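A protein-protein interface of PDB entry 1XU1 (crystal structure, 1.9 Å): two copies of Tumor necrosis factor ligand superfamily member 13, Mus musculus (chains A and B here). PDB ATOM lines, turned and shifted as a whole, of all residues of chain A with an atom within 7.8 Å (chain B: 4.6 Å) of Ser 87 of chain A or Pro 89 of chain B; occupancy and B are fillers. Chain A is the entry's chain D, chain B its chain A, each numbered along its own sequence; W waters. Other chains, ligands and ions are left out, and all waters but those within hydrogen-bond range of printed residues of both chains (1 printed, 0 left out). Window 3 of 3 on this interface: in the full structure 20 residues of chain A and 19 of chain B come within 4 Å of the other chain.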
ATOM      1  N   ASP A  61      24.383   3.334  26.571  1.00  0.00           N
ATOM      2  CA  ASP A  61      23.266   4.273  26.602  1.00  0.00           C
ATOM      3  C   ASP A  61      23.733   5.596  25.966  1.00  0.00           C
ATOM      4  O   ASP A  61      24.782   6.125  26.334  1.00  0.00           O
ATOM      5  CB  ASP A  61      22.868   4.478  28.078  1.00  0.00           C
ATOM      6  CG  ASP A  61      21.432   4.933  28.263  1.00  0.00           C
ATOM      7  OD1 ASP A  61      20.989   5.868  27.557  1.00  0.00           O
ATOM      8  OD2 ASP A  61      20.671   4.424  29.124  1.00  0.00           O
ATOM      9  N   VAL A  62      22.957   6.123  25.015  1.00  0.00           N
ATOM     10  CA  VAL A  62      23.290   7.401  24.370  1.00  0.00           C
ATOM     11  C   VAL A  62      22.836   8.628  25.170  1.00  0.00           C
ATOM     12  O   VAL A  62      23.085   9.761  24.759  1.00  0.00           O
ATOM     13  CB  VAL A  62      22.716   7.503  22.938  1.00  0.00           C
ATOM     14  CG1 VAL A  62      23.225   6.349  22.085  1.00  0.00           C
ATOM     15  CG2 VAL A  62      21.185   7.561  22.950  1.00  0.00           C
ATOM     16  N   THR A  63      22.178   8.420  26.306  1.00  0.00           N
ATOM     17  CA  THR A  63      21.708   9.547  27.113  1.00  0.00           C
ATOM     18  C   THR A  63      22.902  10.454  27.445  1.00  0.00           C
ATOM     19  O   THR A  63      23.959   9.963  27.819  1.00  0.00           O
ATOM     20  CB  THR A  63      21.027   9.040  28.387  1.00  0.00           C
ATOM     21  OG1 THR A  63      19.875   8.245  28.030  1.00  0.00           O
ATOM     22  CG2 THR A  63      20.472  10.207  29.209  1.00  0.00           C
ATOM     23  N   PHE A  64      22.710  11.770  27.310  1.00  0.00           N
ATOM     24  CA  PHE A  64      23.823  12.739  27.237  1.00  0.00           C
ATOM     25  C   PHE A  64      24.869  12.597  28.330  1.00  0.00           C
ATOM     26  O   PHE A  64      26.072  12.684  28.054  1.00  0.00           O
ATOM     27  CB  PHE A  64      23.294  14.188  27.174  1.00  0.00           C
ATOM     28  CG  PHE A  64      22.745  14.707  28.475  1.00  0.00           C
ATOM     29  CD1 PHE A  64      21.587  14.169  29.034  1.00  0.00           C
ATOM     30  CD2 PHE A  64      23.378  15.765  29.138  1.00  0.00           C
ATOM     31  CE1 PHE A  64      21.099  14.643  30.247  1.00  0.00           C
ATOM     32  CE2 PHE A  64      22.885  16.254  30.332  1.00  0.00           C
ATOM     33  CZ  PHE A  64      21.734  15.690  30.893  1.00  0.00           C
ATOM     34  N   THR A  65      24.416  12.380  29.560  1.00  0.00           N
ATOM     35  CA  THR A  65      25.278  11.982  30.660  1.00  0.00           C
ATOM     36  C   THR A  65      24.652  10.810  31.403  1.00  0.00           C
ATOM     37  O   THR A  65      23.441  10.723  31.517  1.00  0.00           O
ATOM     38  CB  THR A  65      25.509  13.144  31.675  1.00  0.00           C
ATOM     39  OG1 THR A  65      24.245  13.722  32.052  1.00  0.00           O
ATOM     40  CG2 THR A  65      26.314  14.286  31.041  1.00  0.00           C
ATOM     41  N   MET A  66      25.496   9.906  31.875  1.00  0.00           N
ATOM     42  CA  MET A  66      25.081   8.805  32.739  1.00  0.00           C
ATOM     43  C   MET A  66      26.010   8.733  33.934  1.00  0.00           C
ATOM     44  O   MET A  66      27.094   9.288  33.929  1.00  0.00           O
ATOM     45  CB  MET A  66      25.106   7.479  31.985  1.00  0.00           C
ATOM     46  CG  MET A  66      24.050   7.372  30.861  1.00  0.00           C
ATOM     47  SD  MET A  66      22.321   7.503  31.404  1.00  0.00           S
ATOM     48  CE  MET A  66      22.112   5.913  32.101  1.00  0.00           C
ATOM     49  N   GLY A  67      25.577   8.019  34.956  1.00  0.00           N
ATOM     50  CA  GLY A  67      26.376   7.863  36.144  1.00  0.00           C
ATOM     51  C   GLY A  67      25.549   7.370  37.305  1.00  0.00           C
ATOM     52  O   GLY A  67      24.338   7.131  37.188  1.00  0.00           O
ATOM     53  N   ILE A  85      30.158  10.531  37.037  1.00  0.00           N
ATOM     54  CA  ILE A  85      29.450  11.095  35.882  1.00  0.00           C
ATOM     55  C   ILE A  85      30.298  10.934  34.616  1.00  0.00           C
ATOM     56  O   ILE A  85      31.486  11.231  34.625  1.00  0.00           O
ATOM     57  CB  ILE A  85      29.129  12.581  36.113  1.00  0.00           C
ATOM     58  CG1 ILE A  85      28.173  12.748  37.313  1.00  0.00           C
ATOM     59  CG2 ILE A  85      28.517  13.202  34.865  1.00  0.00           C
ATOM     60  CD1 ILE A  85      28.103  14.141  37.824  1.00  0.00           C
ATOM     61  N   ARG A  86      29.669  10.471  33.537  1.00  0.00           N
ATOM     62  CA  ARG A  86      30.314  10.340  32.227  1.00  0.00           C
ATOM     63  C   ARG A  86      29.415  10.925  31.139  1.00  0.00           C
ATOM     64  O   ARG A  86      28.226  10.587  31.059  1.00  0.00           O
ATOM     65  CB  ARG A  86      30.558   8.863  31.879  1.00  0.00           C
ATOM     66  CG  ARG A  86      31.650   8.151  32.668  1.00  0.00           C
ATOM     67  CD  ARG A  86      33.077   8.705  32.463  1.00  0.00           C
ATOM     68  NE  ARG A  86      33.660   9.094  33.756  1.00  0.00           N
ATOM     69  CZ  ARG A  86      34.377   8.292  34.540  1.00  0.00           C
ATOM     70  NH1 ARG A  86      34.664   7.052  34.173  1.00  0.00           N
ATOM     71  NH2 ARG A  86      34.836   8.738  35.702  1.00  0.00           N
ATOM     72  N   SER A  87      29.983  11.752  30.270  1.00  0.00           N
ATOM     73  CA  SER A  87      29.281  12.165  29.055  1.00  0.00           C
ATOM     74  C   SER A  87      29.309  11.020  28.062  1.00  0.00           C
ATOM     75  O   SER A  87      30.299  10.289  27.977  1.00  0.00           O
ATOM     76  CB  SER A  87      29.884  13.434  28.446  1.00  0.00           C
ATOM     77  OG  SER A  87      31.290  13.336  28.366  1.00  0.00           O
ATOM     78  N   MET A  88      28.222  10.852  27.314  1.00  0.00           N
ATOM     79  CA  MET A  88      28.102   9.739  26.362  1.00  0.00           C
ATOM     80  C   MET A  88      27.985  10.262  24.937  1.00  0.00           C
ATOM     81  O   MET A  88      27.353  11.289  24.708  1.00  0.00           O
ATOM     82  CB  MET A  88      26.853   8.911  26.668  1.00  0.00           C
ATOM     83  CG  MET A  88      26.712   8.440  28.111  1.00  0.00           C
ATOM     84  SD  MET A  88      27.948   7.234  28.656  1.00  0.00           S
ATOM     85  CE  MET A  88      27.554   5.778  27.616  1.00  0.00           C
ATOM     86  N   PRO A  89      28.544   9.548  23.966  1.00  0.00           N
ATOM     87  CA  PRO A  89      28.337   9.913  22.561  1.00  0.00           C
ATOM     88  C   PRO A  89      26.936   9.557  22.052  1.00  0.00           C
ATOM     89  O   PRO A  89      26.203   8.795  22.680  1.00  0.00           O
ATOM     90  CB  PRO A  89      29.406   9.098  21.818  1.00  0.00           C
ATOM     91  CG  PRO A  89      29.677   7.941  22.684  1.00  0.00           C
ATOM     92  CD  PRO A  89      29.405   8.359  24.108  1.00  0.00           C
ATOM     93  N   SER A  90      26.599  10.087  20.887  1.00  0.00           N
ATOM     94  CA  SER A  90      25.242   9.994  20.348  1.00  0.00           C
ATOM     95  C   SER A  90      24.952   8.703  19.572  1.00  0.00           C
ATOM     96  O   SER A  90      23.785   8.346  19.386  1.00  0.00           O
ATOM     97  CB  SER A  90      24.948  11.212  19.461  1.00  0.00           C
ATOM     98  OG  SER A  90      26.012  11.469  18.555  1.00  0.00           O
ATOM     99  N   ALA A  95      28.430   4.215  22.176  1.00  0.00           N
ATOM    100  CA  ALA A  95      28.026   4.734  23.473  1.00  0.00           C
ATOM    101  C   ALA A  95      28.215   3.718  24.588  1.00  0.00           C
ATOM    102  O   ALA A  95      27.246   3.279  25.205  1.00  0.00           O
ATOM    103  CB  ALA A  95      26.564   5.226  23.421  1.00  0.00           C
ATOM    104  N   TYR A  96      29.474   3.373  24.860  1.00  0.00           N
ATOM    105  CA  TYR A  96      29.841   2.525  25.990  1.00  0.00           C
ATOM    106  C   TYR A  96      30.802   3.307  26.880  1.00  0.00           C
ATOM    107  O   TYR A  96      31.752   3.935  26.390  1.00  0.00           O
ATOM    108  CB  TYR A  96      30.571   1.268  25.525  1.00  0.00           C
ATOM    109  CG  TYR A  96      29.774   0.296  24.674  1.00  0.00           C
ATOM    110  CD1 TYR A  96      29.648   0.495  23.303  1.00  0.00           C
ATOM    111  CD2 TYR A  96      29.195  -0.844  25.231  1.00  0.00           C
ATOM    112  CE1 TYR A  96      28.949  -0.400  22.505  1.00  0.00           C
ATOM    113  CE2 TYR A  96      28.470  -1.745  24.436  1.00  0.00           C
ATOM    114  CZ  TYR A  96      28.366  -1.512  23.074  1.00  0.00           C
ATOM    115  OH  TYR A  96      27.682  -2.372  22.247  1.00  0.00           O
ATOM    116  N   ASN A  97      30.575   3.246  28.184  1.00  0.00           N
ATOM    117  CA  ASN A  97      31.466   3.869  29.152  1.00  0.00           C
ATOM    118  C   ASN A  97      31.260   3.245  30.503  1.00  0.00           C
ATOM    119  O   ASN A  97      30.118   3.129  30.953  1.00  0.00           O
ATOM    120  CB  ASN A  97      31.172   5.369  29.294  1.00  0.00           C
ATOM    121  CG  ASN A  97      31.962   6.233  28.319  1.00  0.00           C
ATOM    122  OD1 ASN A  97      33.171   6.115  28.208  1.00  0.00           O
ATOM    123  ND2 ASN A  97      31.265   7.127  27.621  1.00  0.00           N
ATOM    124  N   CYS A  99      31.953   3.738  34.609  1.00  0.00           N
ATOM    125  CA  CYS A  99      32.032   4.838  35.556  1.00  0.00           C
ATOM    126  C   CYS A  99      32.401   4.253  36.923  1.00  0.00           C
ATOM    127  O   CYS A  99      31.591   3.560  37.538  1.00  0.00           O
ATOM    128  CB  CYS A  99      30.683   5.554  35.624  1.00  0.00           C
ATOM    129  SG  CYS A  99      30.840   7.303  36.031  1.00  0.00           S
ATOM    130  N   VAL B  62      34.206  22.906  29.131  1.00  0.00           N
ATOM    131  CA  VAL B  62      34.295  22.453  27.738  1.00  0.00           C
ATOM    132  C   VAL B  62      35.741  22.381  27.230  1.00  0.00           C
ATOM    133  O   VAL B  62      35.968  22.055  26.070  1.00  0.00           O
ATOM    134  CB  VAL B  62      33.440  23.306  26.751  1.00  0.00           C
ATOM    135  CG1 VAL B  62      31.969  23.242  27.109  1.00  0.00           C
ATOM    136  CG2 VAL B  62      33.925  24.755  26.656  1.00  0.00           C
ATOM    137  N   SER B  87      38.698  13.558  28.147  1.00  0.00           N
ATOM    138  CA  SER B  87      38.343  14.413  27.016  1.00  0.00           C
ATOM    139  C   SER B  87      36.937  14.953  27.310  1.00  0.00           C
ATOM    140  O   SER B  87      36.101  14.240  27.868  1.00  0.00           O
ATOM    141  CB  SER B  87      38.404  13.609  25.718  1.00  0.00           C
ATOM    142  OG  SER B  87      37.899  14.357  24.635  1.00  0.00           O
ATOM    143  N   MET B  88      36.695  16.212  26.971  1.00  0.00           N
ATOM    144  CA  MET B  88      35.417  16.859  27.233  1.00  0.00           C
ATOM    145  C   MET B  88      34.722  17.238  25.928  1.00  0.00           C
ATOM    146  O   MET B  88      35.366  17.613  24.955  1.00  0.00           O
ATOM    147  CB  MET B  88      35.603  18.122  28.088  1.00  0.00           C
ATOM    148  CG  MET B  88      36.398  17.914  29.357  1.00  0.00           C
ATOM    149  SD  MET B  88      35.581  16.882  30.606  1.00  0.00           S
ATOM    150  CE  MET B  88      34.164  17.845  31.058  1.00  0.00           C
ATOM    151  N   PRO B  89      33.399  17.136  25.912  1.00  0.00           N
ATOM    152  CA  PRO B  89      32.619  17.640  24.777  1.00  0.00           C
ATOM    153  C   PRO B  89      32.585  19.176  24.709  1.00  0.00           C
ATOM    154  O   PRO B  89      32.858  19.867  25.693  1.00  0.00           O
ATOM    155  CB  PRO B  89      31.228  17.046  24.997  1.00  0.00           C
ATOM    156  CG  PRO B  89      31.177  16.561  26.364  1.00  0.00           C
ATOM    157  CD  PRO B  89      32.563  16.499  26.940  1.00  0.00           C
ATOM    158  N   SER B  90      32.254  19.698  23.538  1.00  0.00           N
ATOM    159  CA  SER B  90      32.252  21.148  23.299  1.00  0.00           C
ATOM    160  C   SER B  90      30.940  21.859  23.717  1.00  0.00           C
ATOM    161  O   SER B  90      30.874  23.101  23.782  1.00  0.00           O
ATOM    162  CB  SER B  90      32.556  21.413  21.826  1.00  0.00           C
ATOM    163  OG  SER B  90      31.556  20.862  20.992  1.00  0.00           O
ATOM    164  N   ASP B  91      29.904  21.086  24.016  1.00  0.00           N
ATOM    165  CA  ASP B  91      28.622  21.654  24.441  1.00  0.00           C
ATOM    166  C   ASP B  91      28.565  21.693  25.968  1.00  0.00           C
ATOM    167  O   ASP B  91      28.731  20.650  26.608  1.00  0.00           O
ATOM    168  CB  ASP B  91      27.454  20.822  23.896  1.00  0.00           C
ATOM    169  CG  ASP B  91      26.113  21.307  24.404  1.00  0.00           C
ATOM    170  OD1 ASP B  91      25.763  22.490  24.161  1.00  0.00           O
ATOM    171  OD2 ASP B  91      25.342  20.575  25.060  1.00  0.00           O
ATOM    172  N   ARG B  94      26.459  19.091  27.979  1.00  0.00           N
ATOM    173  CA  ARG B  94      27.024  17.746  27.943  1.00  0.00           C
ATOM    174  C   ARG B  94      28.363  17.635  28.675  1.00  0.00           C
ATOM    175  O   ARG B  94      28.815  16.531  28.935  1.00  0.00           O
ATOM    176  CB  ARG B  94      27.289  17.309  26.497  1.00  0.00           C
ATOM    177  CG  ARG B  94      26.075  16.949  25.684  1.00  0.00           C
ATOM    178  CD  ARG B  94      26.424  16.633  24.224  1.00  0.00           C
ATOM    179  NE  ARG B  94      25.262  16.142  23.498  1.00  0.00           N
ATOM    180  CZ  ARG B  94      24.335  16.928  22.962  1.00  0.00           C
ATOM    181  NH1 ARG B  94      24.432  18.246  23.067  1.00  0.00           N
ATOM    182  NH2 ARG B  94      23.308  16.395  22.308  1.00  0.00           N
ATOM    183  N   ALA B  95      29.005  18.763  28.974  1.00  0.00           N
ATOM    184  CA  ALA B  95      30.405  18.770  29.414  1.00  0.00           C
ATOM    185  C   ALA B  95      30.553  18.561  30.923  1.00  0.00           C
ATOM    186  O   ALA B  95      31.082  19.414  31.622  1.00  0.00           O
ATOM    187  CB  ALA B  95      31.081  20.061  28.987  1.00  0.00           C
ATOM    188  N   TYR B  96      30.073  17.417  31.403  1.00  0.00           N
ATOM    189  CA  TYR B  96      30.250  16.969  32.780  1.00  0.00           C
ATOM    190  C   TYR B  96      30.986  15.625  32.741  1.00  0.00           C
ATOM    191  O   TYR B  96      30.572  14.703  32.019  1.00  0.00           O
ATOM    192  CB  TYR B  96      28.880  16.764  33.457  1.00  0.00           C
ATOM    193  CG  TYR B  96      28.006  17.988  33.648  1.00  0.00           C
ATOM    194  CD1 TYR B  96      27.200  18.455  32.620  1.00  0.00           C
ATOM    195  CD2 TYR B  96      27.951  18.655  34.875  1.00  0.00           C
ATOM    196  CE1 TYR B  96      26.376  19.554  32.791  1.00  0.00           C
ATOM    197  CE2 TYR B  96      27.124  19.774  35.057  1.00  0.00           C
ATOM    198  CZ  TYR B  96      26.331  20.205  34.024  1.00  0.00           C
ATOM    199  OH  TYR B  96      25.517  21.312  34.156  1.00  0.00           O
ATOM    200  N   ASN B  97      32.071  15.497  33.509  1.00  0.00           N
ATOM    201  CA  ASN B  97      32.801  14.248  33.623  1.00  0.00           C
ATOM    202  C   ASN B  97      33.550  14.246  34.954  1.00  0.00           C
ATOM    203  O   ASN B  97      34.248  15.226  35.274  1.00  0.00           O
ATOM    204  CB  ASN B  97      33.849  14.119  32.497  1.00  0.00           C
ATOM    205  CG  ASN B  97      33.319  13.437  31.236  1.00  0.00           C
ATOM    206  OD1 ASN B  97      32.719  12.364  31.285  1.00  0.00           O
ATOM    207  ND2 ASN B  97      33.571  14.061  30.093  1.00  0.00           N
HETATM  208  O   HOH W   1      32.958  10.310  29.115  1.00  0.00           O
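Of the 10 printed residues of chain B, 4 touch a printed residue of chain A. Hydrophobic or aromatic side chains of chain B that line the printed part of chain A: Pro 89 and Tyr 96. Hydrophobic or aromatic side chains of chain A that line the printed part of chain B: Ile 85. Among the printed residues, 8 pairs touch across the chains. Among the printed residues, no Asp or Glu carboxylate lies within 4 Å of a Lys or Arg side-chain nitrogen of the other chain.
Thr 65 of chain A touches Arg 94 of chain B (CG2 to O, 3.97 Å). CG2 of Ile 85 of chain A touches O of Tyr 96 of chain B, at 3.8 Å. Ile 85 of chain A touches Asn 97 of chain B (O to CA, 3.4 Å). Asn 97 of chain B touches Arg 86 of chain A. Ser 87 of chain A touches Pro 89 of chain B. CB of Ser 87 of chain A touches O of Arg 94 of chain B, at 3.3 Å.
Of the printed residues of chain B, Thr 65 of chain A touches Arg 94. Of the printed residues of chain B, Arg 86 of chain A touches Asn 97 (3.3 Å). Ser 87 of chain A touches four residues of chain B. Ser 90 of chain A touches none of the printed residues of chain B. Val 62 of chain B touches none of the printed residues of chain A. Of the printed residues of chain A, Pro 89 of chain B touches Ser 87 (3.7 Å). Of the printed residues of chain A, Arg 94 of chain B touches Thr 65 and Ser 87. The nearest printed residue of chain B that does not touch Ser 87 of chain A is Ser 87 of chain B (4.9 Å).
The side-chain amide nitrogen (ND2) of Asn 97 of chain B sits at hydrogen-bond distance from the side-chain hydroxyl (OG) of Ser 87 of chain A. O of Tyr 96 of chain B is in hydrogen-bond range of N of Ser 87 of chain A (3.5 Å).
Water W1 bridges O of Ser 87 of chain A and OD1 of Asn 97 of chain B.
Ser 87 of chain A touches Pro 89 of chain B, but with the chains exchanged Pro 89 of chain A does not touch Ser 87 of chain B (9.7 Å). Ser 87 of chain A touches Tyr 96 of chain B, but with the chains exchanged Tyr 96 of chain A does not touch Ser 87 of chain B (11.3 Å). Ser 87 of chain A touches Asn 97 of chain B, but with the chains exchanged Asn 97 of chain A does not touch Ser 87 of chain B (8.6 Å). 8 positions are printed for both chains. Of the 8 pairs that touch across the chains among the printed residues, none has its exchanged pair printed and touching as well.
The backbone NH (N) of Arg 86 of chain A is in hydrogen-bond range of the backbone carbonyl oxygen (O) of Met 66 of chain A. The side-chain amide nitrogen (ND2) of Asn 97 of chain B sits at hydrogen-bond distance from the backbone carbonyl oxygen (O) of Ser 87 of chain B (3.4 Å). The guanidinium group of Arg 94 of chain B lies within salt-bridge range of the side-chain carboxylate of Asp 91 of chain B (3.2 Å). N of Ile 85 of chain A sits at hydrogen-bond distance from SG of Cys 99 of chain A. The side-chain sulfur of Met 88 of chain B lies within hydrogen-bond range of the side-chain amide nitrogen of Asn 97 of chain B (3.5 Å). The side-chain amide nitrogen (ND2) of Asn 97 of chain A lies within hydrogen-bond range of the backbone carbonyl oxygen (O) of Ser 87 of chain A, 3.3 Å away.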
